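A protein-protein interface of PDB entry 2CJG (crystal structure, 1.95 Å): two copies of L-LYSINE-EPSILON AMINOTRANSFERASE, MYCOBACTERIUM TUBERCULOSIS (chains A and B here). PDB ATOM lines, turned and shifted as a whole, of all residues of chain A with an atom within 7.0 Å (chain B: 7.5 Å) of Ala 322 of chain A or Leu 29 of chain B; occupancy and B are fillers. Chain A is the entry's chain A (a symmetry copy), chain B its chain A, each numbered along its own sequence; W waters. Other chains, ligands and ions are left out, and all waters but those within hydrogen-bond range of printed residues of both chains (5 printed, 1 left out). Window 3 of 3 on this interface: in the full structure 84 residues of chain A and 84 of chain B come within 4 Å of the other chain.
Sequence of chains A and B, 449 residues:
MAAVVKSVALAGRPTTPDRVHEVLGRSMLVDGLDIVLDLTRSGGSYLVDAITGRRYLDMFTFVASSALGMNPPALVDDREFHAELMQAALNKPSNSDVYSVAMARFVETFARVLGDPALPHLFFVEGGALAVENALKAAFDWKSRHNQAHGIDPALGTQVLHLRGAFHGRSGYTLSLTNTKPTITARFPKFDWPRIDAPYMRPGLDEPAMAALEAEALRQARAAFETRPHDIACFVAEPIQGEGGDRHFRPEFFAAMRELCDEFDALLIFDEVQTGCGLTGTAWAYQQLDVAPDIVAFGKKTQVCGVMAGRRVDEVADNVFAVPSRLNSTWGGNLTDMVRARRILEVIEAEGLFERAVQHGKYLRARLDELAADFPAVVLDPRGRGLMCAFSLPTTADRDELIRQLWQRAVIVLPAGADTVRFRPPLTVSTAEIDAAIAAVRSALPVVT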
ATOM      1  N   SER A  96      27.973   2.568  -4.935  1.00  0.00           N
ATOM      2  CA  SER A  96      28.427   1.215  -4.565  1.00  0.00           C
ATOM      3  C   SER A  96      27.573   0.629  -3.435  1.00  0.00           C
ATOM      4  O   SER A  96      27.263  -0.548  -3.458  1.00  0.00           O
ATOM      5  CB  SER A  96      29.901   1.260  -4.120  1.00  0.00           C
ATOM      6  OG  SER A  96      30.739   1.809  -5.137  1.00  0.00           O
ATOM      7  N   TYR A  99      21.696   2.946  -3.117  1.00  0.00           N
ATOM      8  CA  TYR A  99      20.988   2.986  -4.398  1.00  0.00           C
ATOM      9  C   TYR A  99      19.939   4.067  -4.411  1.00  0.00           C
ATOM     10  O   TYR A  99      19.476   4.490  -3.359  1.00  0.00           O
ATOM     11  CB  TYR A  99      20.337   1.631  -4.684  1.00  0.00           C
ATOM     12  CG  TYR A  99      21.328   0.502  -4.576  1.00  0.00           C
ATOM     13  CD1 TYR A  99      22.615   0.610  -5.143  1.00  0.00           C
ATOM     14  CD2 TYR A  99      21.007  -0.655  -3.893  1.00  0.00           C
ATOM     15  CE1 TYR A  99      23.550  -0.428  -5.018  1.00  0.00           C
ATOM     16  CE2 TYR A  99      21.930  -1.682  -3.761  1.00  0.00           C
ATOM     17  CZ  TYR A  99      23.180  -1.563  -4.324  1.00  0.00           C
ATOM     18  OH  TYR A  99      24.041  -2.624  -4.190  1.00  0.00           O
ATOM     19  N   HIS A 121      25.889  -8.306 -17.542  1.00  0.00           N
ATOM     20  CA  HIS A 121      26.530  -7.793 -16.303  1.00  0.00           C
ATOM     21  C   HIS A 121      27.096  -6.406 -16.561  1.00  0.00           C
ATOM     22  O   HIS A 121      27.945  -6.229 -17.461  1.00  0.00           O
ATOM     23  CB  HIS A 121      27.666  -8.688 -15.863  1.00  0.00           C
ATOM     24  CG  HIS A 121      27.272 -10.121 -15.746  1.00  0.00           C
ATOM     25  ND1 HIS A 121      26.321 -10.551 -14.849  1.00  0.00           N
ATOM     26  CD2 HIS A 121      27.663 -11.216 -16.445  1.00  0.00           C
ATOM     27  CE1 HIS A 121      26.153 -11.856 -14.987  1.00  0.00           C
ATOM     28  NE2 HIS A 121      26.953 -12.283 -15.948  1.00  0.00           N
ATOM     29  N   LEU A 122      26.649  -5.441 -15.760  1.00  0.00           N
ATOM     30  CA  LEU A 122      27.093  -4.059 -15.890  1.00  0.00           C
ATOM     31  C   LEU A 122      27.876  -3.658 -14.639  1.00  0.00           C
ATOM     32  O   LEU A 122      27.505  -4.045 -13.522  1.00  0.00           O
ATOM     33  CB  LEU A 122      25.879  -3.151 -16.058  1.00  0.00           C
ATOM     34  CG  LEU A 122      25.336  -2.817 -17.466  1.00  0.00           C
ATOM     35  CD1 LEU A 122      25.767  -3.733 -18.570  1.00  0.00           C
ATOM     36  CD2 LEU A 122      23.855  -2.521 -17.497  1.00  0.00           C
ATOM     37  N   VAL A 316      32.321 -19.473 -15.488  1.00  0.00           N
ATOM     38  CA  VAL A 316      32.979 -19.582 -14.189  1.00  0.00           C
ATOM     39  C   VAL A 316      31.939 -18.957 -13.250  1.00  0.00           C
ATOM     40  O   VAL A 316      31.731 -17.728 -13.254  1.00  0.00           O
ATOM     41  CB  VAL A 316      34.328 -18.804 -14.193  1.00  0.00           C
ATOM     42  CG1 VAL A 316      34.843 -18.550 -12.790  1.00  0.00           C
ATOM     43  CG2 VAL A 316      35.378 -19.530 -15.053  1.00  0.00           C
ATOM     44  N   ALA A 317      31.270 -19.801 -12.479  1.00  0.00           N
ATOM     45  CA  ALA A 317      30.135 -19.374 -11.692  1.00  0.00           C
ATOM     46  C   ALA A 317      30.507 -18.363 -10.590  1.00  0.00           C
ATOM     47  O   ALA A 317      29.660 -17.573 -10.223  1.00  0.00           O
ATOM     48  CB  ALA A 317      29.401 -20.588 -11.081  1.00  0.00           C
ATOM     49  N   ASP A 318      31.746 -18.416 -10.090  1.00  0.00           N
ATOM     50  CA  ASP A 318      32.204 -17.492  -9.031  1.00  0.00           C
ATOM     51  C   ASP A 318      33.113 -16.396  -9.591  1.00  0.00           C
ATOM     52  O   ASP A 318      34.111 -16.030  -8.987  1.00  0.00           O
ATOM     53  CB  ASP A 318      32.852 -18.254  -7.862  1.00  0.00           C
ATOM     54  CG  ASP A 318      33.821 -19.346  -8.322  1.00  0.00           C
ATOM     55  OD1 ASP A 318      33.977 -19.610  -9.535  1.00  0.00           O
ATOM     56  OD2 ASP A 318      34.427 -19.980  -7.453  1.00  0.00           O
ATOM     57  N   ASN A 319      32.746 -15.887 -10.765  1.00  0.00           N
ATOM     58  CA  ASN A 319      33.426 -14.763 -11.400  1.00  0.00           C
ATOM     59  C   ASN A 319      33.186 -13.421 -10.619  1.00  0.00           C
ATOM     60  O   ASN A 319      32.404 -13.370  -9.659  1.00  0.00           O
ATOM     61  CB  ASN A 319      32.947 -14.656 -12.865  1.00  0.00           C
ATOM     62  CG  ASN A 319      31.498 -14.222 -12.973  1.00  0.00           C
ATOM     63  OD1 ASN A 319      31.154 -13.076 -12.649  1.00  0.00           O
ATOM     64  ND2 ASN A 319      30.622 -15.136 -13.396  1.00  0.00           N
ATOM     65  N   VAL A 320      33.860 -12.341 -11.036  1.00  0.00           N
ATOM     66  CA  VAL A 320      33.865 -11.088 -10.240  1.00  0.00           C
ATOM     67  C   VAL A 320      32.525 -10.390 -10.252  1.00  0.00           C
ATOM     68  O   VAL A 320      32.291  -9.504  -9.437  1.00  0.00           O
ATOM     69  CB  VAL A 320      34.975 -10.086 -10.656  1.00  0.00           C
ATOM     70  CG1 VAL A 320      36.329 -10.649 -10.371  1.00  0.00           C
ATOM     71  CG2 VAL A 320      34.836  -9.719 -12.142  1.00  0.00           C
ATOM     72  N   PHE A 321      31.645 -10.760 -11.175  1.00  0.00           N
ATOM     73  CA  PHE A 321      30.314 -10.165 -11.221  1.00  0.00           C
ATOM     74  C   PHE A 321      29.359 -10.898 -10.319  1.00  0.00           C
ATOM     75  O   PHE A 321      28.289 -10.394 -10.024  1.00  0.00           O
ATOM     76  CB  PHE A 321      29.808 -10.080 -12.665  1.00  0.00           C
ATOM     77  CG  PHE A 321      30.770  -9.351 -13.555  1.00  0.00           C
ATOM     78  CD1 PHE A 321      30.863  -7.959 -13.493  1.00  0.00           C
ATOM     79  CD2 PHE A 321      31.637 -10.046 -14.385  1.00  0.00           C
ATOM     80  CE1 PHE A 321      31.792  -7.279 -14.272  1.00  0.00           C
ATOM     81  CE2 PHE A 321      32.565  -9.366 -15.185  1.00  0.00           C
ATOM     82  CZ  PHE A 321      32.641  -7.994 -15.111  1.00  0.00           C
ATOM     83  N   ALA A 322      29.774 -12.075  -9.843  1.00  0.00           N
ATOM     84  CA  ALA A 322      28.913 -12.938  -9.042  1.00  0.00           C
ATOM     85  C   ALA A 322      29.295 -12.940  -7.553  1.00  0.00           C
ATOM     86  O   ALA A 322      28.509 -13.316  -6.723  1.00  0.00           O
ATOM     87  CB  ALA A 322      28.958 -14.342  -9.603  1.00  0.00           C
ATOM     88  N   VAL A 323      30.502 -12.506  -7.225  1.00  0.00           N
ATOM     89  CA  VAL A 323      31.053 -12.608  -5.880  1.00  0.00           C
ATOM     90  C   VAL A 323      31.203 -11.169  -5.368  1.00  0.00           C
ATOM     91  O   VAL A 323      31.819 -10.343  -6.052  1.00  0.00           O
ATOM     92  CB  VAL A 323      32.438 -13.307  -5.939  1.00  0.00           C
ATOM     93  CG1 VAL A 323      33.242 -13.146  -4.626  1.00  0.00           C
ATOM     94  CG2 VAL A 323      32.267 -14.772  -6.324  1.00  0.00           C
ATOM     95  N   PRO A 324      30.671 -10.869  -4.166  1.00  0.00           N
ATOM     96  CA  PRO A 324      30.820  -9.488  -3.661  1.00  0.00           C
ATOM     97  C   PRO A 324      32.271  -9.070  -3.360  1.00  0.00           C
ATOM     98  O   PRO A 324      33.128  -9.898  -3.008  1.00  0.00           O
ATOM     99  CB  PRO A 324      29.992  -9.489  -2.364  1.00  0.00           C
ATOM    100  CG  PRO A 324      30.017 -10.914  -1.930  1.00  0.00           C
ATOM    101  CD  PRO A 324      29.946 -11.720  -3.206  1.00  0.00           C
ATOM    102  N   SER A 325      32.511  -7.774  -3.540  1.00  0.00           N
ATOM    103  CA  SER A 325      33.761  -7.106  -3.173  1.00  0.00           C
ATOM    104  C   SER A 325      35.003  -7.426  -4.004  1.00  0.00           C
ATOM    105  O   SER A 325      36.096  -7.016  -3.629  1.00  0.00           O
ATOM    106  CB  SER A 325      34.052  -7.268  -1.671  1.00  0.00           C
ATOM    107  OG  SER A 325      34.519  -6.021  -1.138  1.00  0.00           O
ATOM    108  N   ARG A 326      34.851  -8.097  -5.151  1.00  0.00           N
ATOM    109  CA  ARG A 326      36.023  -8.350  -6.005  1.00  0.00           C
ATOM    110  C   ARG A 326      36.387  -7.117  -6.852  1.00  0.00           C
ATOM    111  O   ARG A 326      37.560  -6.853  -7.106  1.00  0.00           O
ATOM    112  CB  ARG A 326      35.778  -9.571  -6.914  1.00  0.00           C
ATOM    113  CG  ARG A 326      35.627 -10.889  -6.148  1.00  0.00           C
ATOM    114  CD  ARG A 326      36.967 -11.337  -5.625  1.00  0.00           C
ATOM    115  NE  ARG A 326      37.796 -11.825  -6.721  1.00  0.00           N
ATOM    116  CZ  ARG A 326      39.123 -11.718  -6.785  1.00  0.00           C
ATOM    117  NH1 ARG A 326      39.812 -11.103  -5.814  1.00  0.00           N
ATOM    118  NH2 ARG A 326      39.762 -12.226  -7.827  1.00  0.00           N
ATOM    119  N   LEU B  24      17.956  -2.887 -10.537  1.00  0.00           N
ATOM    120  CA  LEU B  24      19.419  -2.977 -10.498  1.00  0.00           C
ATOM    121  C   LEU B  24      19.886  -4.426 -10.509  1.00  0.00           C
ATOM    122  O   LEU B  24      20.934  -4.744 -11.102  1.00  0.00           O
ATOM    123  CB  LEU B  24      20.005  -2.262  -9.268  1.00  0.00           C
ATOM    124  CG  LEU B  24      19.774  -0.744  -9.189  1.00  0.00           C
ATOM    125  CD1 LEU B  24      20.339  -0.213  -7.874  1.00  0.00           C
ATOM    126  CD2 LEU B  24      20.386  -0.027 -10.373  1.00  0.00           C
ATOM    127  N   GLY B  25      19.125  -5.297  -9.842  1.00  0.00           N
ATOM    128  CA  GLY B  25      19.504  -6.701  -9.695  1.00  0.00           C
ATOM    129  C   GLY B  25      19.513  -7.449 -11.017  1.00  0.00           C
ATOM    130  O   GLY B  25      20.168  -8.454 -11.138  1.00  0.00           O
ATOM    131  N   ARG B  26      18.836  -6.940 -12.028  1.00  0.00           N
ATOM    132  CA  ARG B  26      18.943  -7.551 -13.377  1.00  0.00           C
ATOM    133  C   ARG B  26      20.334  -7.387 -14.041  1.00  0.00           C
ATOM    134  O   ARG B  26      20.681  -8.137 -14.976  1.00  0.00           O
ATOM    135  CB  ARG B  26      17.863  -6.985 -14.294  1.00  0.00           C
ATOM    136  CG  ARG B  26      16.435  -7.075 -13.723  1.00  0.00           C
ATOM    137  CD  ARG B  26      15.431  -6.782 -14.817  1.00  0.00           C
ATOM    138  NE  ARG B  26      14.155  -6.230 -14.332  1.00  0.00           N
ATOM    139  CZ  ARG B  26      13.693  -5.013 -14.649  1.00  0.00           C
ATOM    140  NH1 ARG B  26      14.397  -4.197 -15.442  1.00  0.00           N
ATOM    141  NH2 ARG B  26      12.521  -4.609 -14.175  1.00  0.00           N
ATOM    142  N   SER B  27      21.121  -6.414 -13.567  1.00  0.00           N
ATOM    143  CA  SER B  27      22.352  -6.022 -14.245  1.00  0.00           C
ATOM    144  C   SER B  27      23.582  -6.119 -13.362  1.00  0.00           C
ATOM    145  O   SER B  27      24.696  -6.180 -13.874  1.00  0.00           O
ATOM    146  CB  SER B  27      22.232  -4.565 -14.699  1.00  0.00           C
ATOM    147  OG  SER B  27      21.293  -4.437 -15.726  1.00  0.00           O
ATOM    148  N   MET B  28      23.384  -6.072 -12.044  1.00  0.00           N
ATOM    149  CA  MET B  28      24.501  -5.967 -11.107  1.00  0.00           C
ATOM    150  C   MET B  28      24.256  -6.817  -9.893  1.00  0.00           C
ATOM    151  O   MET B  28      23.121  -7.165  -9.582  1.00  0.00           O
ATOM    152  CB  MET B  28      24.661  -4.522 -10.590  1.00  0.00           C
ATOM    153  CG  MET B  28      24.106  -3.411 -11.481  1.00  0.00           C
ATOM    154  SD  MET B  28      24.523  -1.729 -10.907  1.00  0.00           S
ATOM    155  CE  MET B  28      24.650  -2.038  -9.169  1.00  0.00           C
ATOM    156  N   LEU B  29      25.333  -7.095  -9.181  1.00  0.00           N
ATOM    157  CA  LEU B  29      25.253  -7.667  -7.858  1.00  0.00           C
ATOM    158  C   LEU B  29      24.747  -6.600  -6.865  1.00  0.00           C
ATOM    159  O   LEU B  29      25.378  -5.557  -6.705  1.00  0.00           O
ATOM    160  CB  LEU B  29      26.652  -8.165  -7.481  1.00  0.00           C
ATOM    161  CG  LEU B  29      26.785  -9.020  -6.241  1.00  0.00           C
ATOM    162  CD1 LEU B  29      26.091 -10.322  -6.515  1.00  0.00           C
ATOM    163  CD2 LEU B  29      28.252  -9.222  -5.986  1.00  0.00           C
ATOM    164  N   VAL B  30      23.607  -6.819  -6.230  1.00  0.00           N
ATOM    165  CA  VAL B  30      23.087  -5.762  -5.339  1.00  0.00           C
ATOM    166  C   VAL B  30      23.392  -6.071  -3.871  1.00  0.00           C
ATOM    167  O   VAL B  30      22.584  -6.645  -3.149  1.00  0.00           O
ATOM    168  CB  VAL B  30      21.587  -5.332  -5.640  1.00  0.00           C
ATOM    169  CG1 VAL B  30      20.827  -6.399  -6.395  1.00  0.00           C
ATOM    170  CG2 VAL B  30      20.823  -4.935  -4.380  1.00  0.00           C
ATOM    171  N   ASP B  31      24.582  -5.706  -3.438  1.00  0.00           N
ATOM    172  CA  ASP B  31      24.983  -6.044  -2.082  1.00  0.00           C
ATOM    173  C   ASP B  31      25.065  -4.824  -1.135  1.00  0.00           C
ATOM    174  O   ASP B  31      25.617  -4.941  -0.041  1.00  0.00           O
ATOM    175  CB  ASP B  31      26.310  -6.799  -2.115  1.00  0.00           C
ATOM    176  CG  ASP B  31      27.442  -5.958  -2.703  1.00  0.00           C
ATOM    177  OD1 ASP B  31      27.161  -5.087  -3.569  1.00  0.00           O
ATOM    178  OD2 ASP B  31      28.614  -6.151  -2.283  1.00  0.00           O
ATOM    179  N   GLY B  32      24.509  -3.679  -1.537  1.00  0.00           N
ATOM    180  CA  GLY B  32      24.530  -2.484  -0.689  1.00  0.00           C
ATOM    181  C   GLY B  32      23.412  -2.480   0.347  1.00  0.00           C
ATOM    182  O   GLY B  32      22.802  -3.522   0.632  1.00  0.00           O
HETATM  183  O   HOH W   1      27.835  -2.575  -1.570  1.00  0.00           O
HETATM  184  O   HOH W   2      27.682  -6.691 -12.660  1.00  0.00           O
HETATM  185  O   HOH W   3      23.338  -9.536 -14.751  1.00  0.00           O
HETATM  186  O   HOH W   4      27.980  -7.035 -10.050  1.00  0.00           O
HETATM  187  O   HOH W   5      25.928  -8.910 -12.458  1.00  0.00           O
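O of Ser 27 of chain B sits at hydrogen-bond distance from N of Leu 122 of chain A (2.8 Å).
The backbone NH of Asp 31 of chain B sits at hydrogen-bond distance from the side-chain hydroxyl of Tyr 99 of chain A, at 3.2 Å.
The side-chain hydroxyl (OH) of Tyr 99 of chain A sits at hydrogen-bond distance from the backbone NH (N) of Gly 32 of chain B, at 2.9 Å.
N of Phe 321 of chain A is in hydrogen-bond range of OD1 of Asn 319 of chain A (2.8 Å).
The backbone NH (N) of Ala 322 of chain A lies within hydrogen-bond range of the side-chain amide oxygen (OD1) of Asn 319 of chain A (3.3 Å).
Tyr 99 of chain A touches Leu 24 of chain B.
Val 30 of chain B touches Tyr 99 of chain A.
Ser 27 of chain B touches His 121 of chain A (O to CA, 3.4 Å).
Leu 29 of chain B touches Phe 321 of chain A.
O of Ala 322 of chain A touches CD1 of Leu 29 of chain B (3.9 Å).
C of Val 323 of chain A touches CD2 of Leu 29 of chain B, at 3.6 Å.
Leu 29 of chain B touches Pro 324 of chain A (CD2 to N, 3.4 Å).
Asp 31 of chain B touches Pro 324 of chain A (OD2 to CB, 3.6 Å).
Leu 29 of chain B touches four residues of chain A.
Of the printed residues of chain A, Ser 27 of chain B touches His 121 and Leu 122.
Of the printed residues of chain A, Asp 31 of chain B touches Tyr 99 (3.2 Å) and Pro 324 (3.6 Å).
Of the printed residues of chain B, Tyr 99 of chain A touches Leu 24, Val 30, Asp 31 and Gly 32.
Of the printed residues of chain B, His 121 of chain A touches Ser 27.
Val 320 of chain A touches none of the printed residues of chain B.
The nearest printed residue of chain B that does not touch Ala 322 of chain A is Met 28 of chain B (7.6 Å).
The nearest residue of chain A that does not touch Leu 29 of chain B is Tyr 99 of chain A (4.1 Å).
The nearest printed residue of chain B that does not touch Phe 321 of chain A is Met 28 of chain B (5.4 Å).
Printed residues of chain B that touch a printed residue of chain A: Leu 24, Ser 27, Leu 29, Val 30, Asp 31 and Gly 32.
Hydrophobic or aromatic side chains of chain A that line the printed part of chain B: Tyr 99, Leu 122 and Pro 324.
Among the printed residues, 11 pairs touch across the chains.
No position is printed for both chains.
Water W4 lies within hydrogen-bond range of the backbone NH (N) of Leu 29 of chain B and the backbone carbonyl oxygen (O) of Phe 321 of chain A.
Water W2 lies within hydrogen-bond range of O of Leu 122 of chain A (2.8 Å) and O of Ser 27 of chain B (3.3 Å).
Water W1 bridges O of Ser 96 of chain A (2.8 Å) and OD1 of Asp 31 of chain B (3.3 Å).
Water W5 bridges ND1 of His 121 of chain A (2.9 Å) and O of Ser 27 of chain B (3.3 Å).
Water W3 bridges O of Arg 26 of chain B (3.0 Å) and ND1 of His 121 of chain A (3.2 Å).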
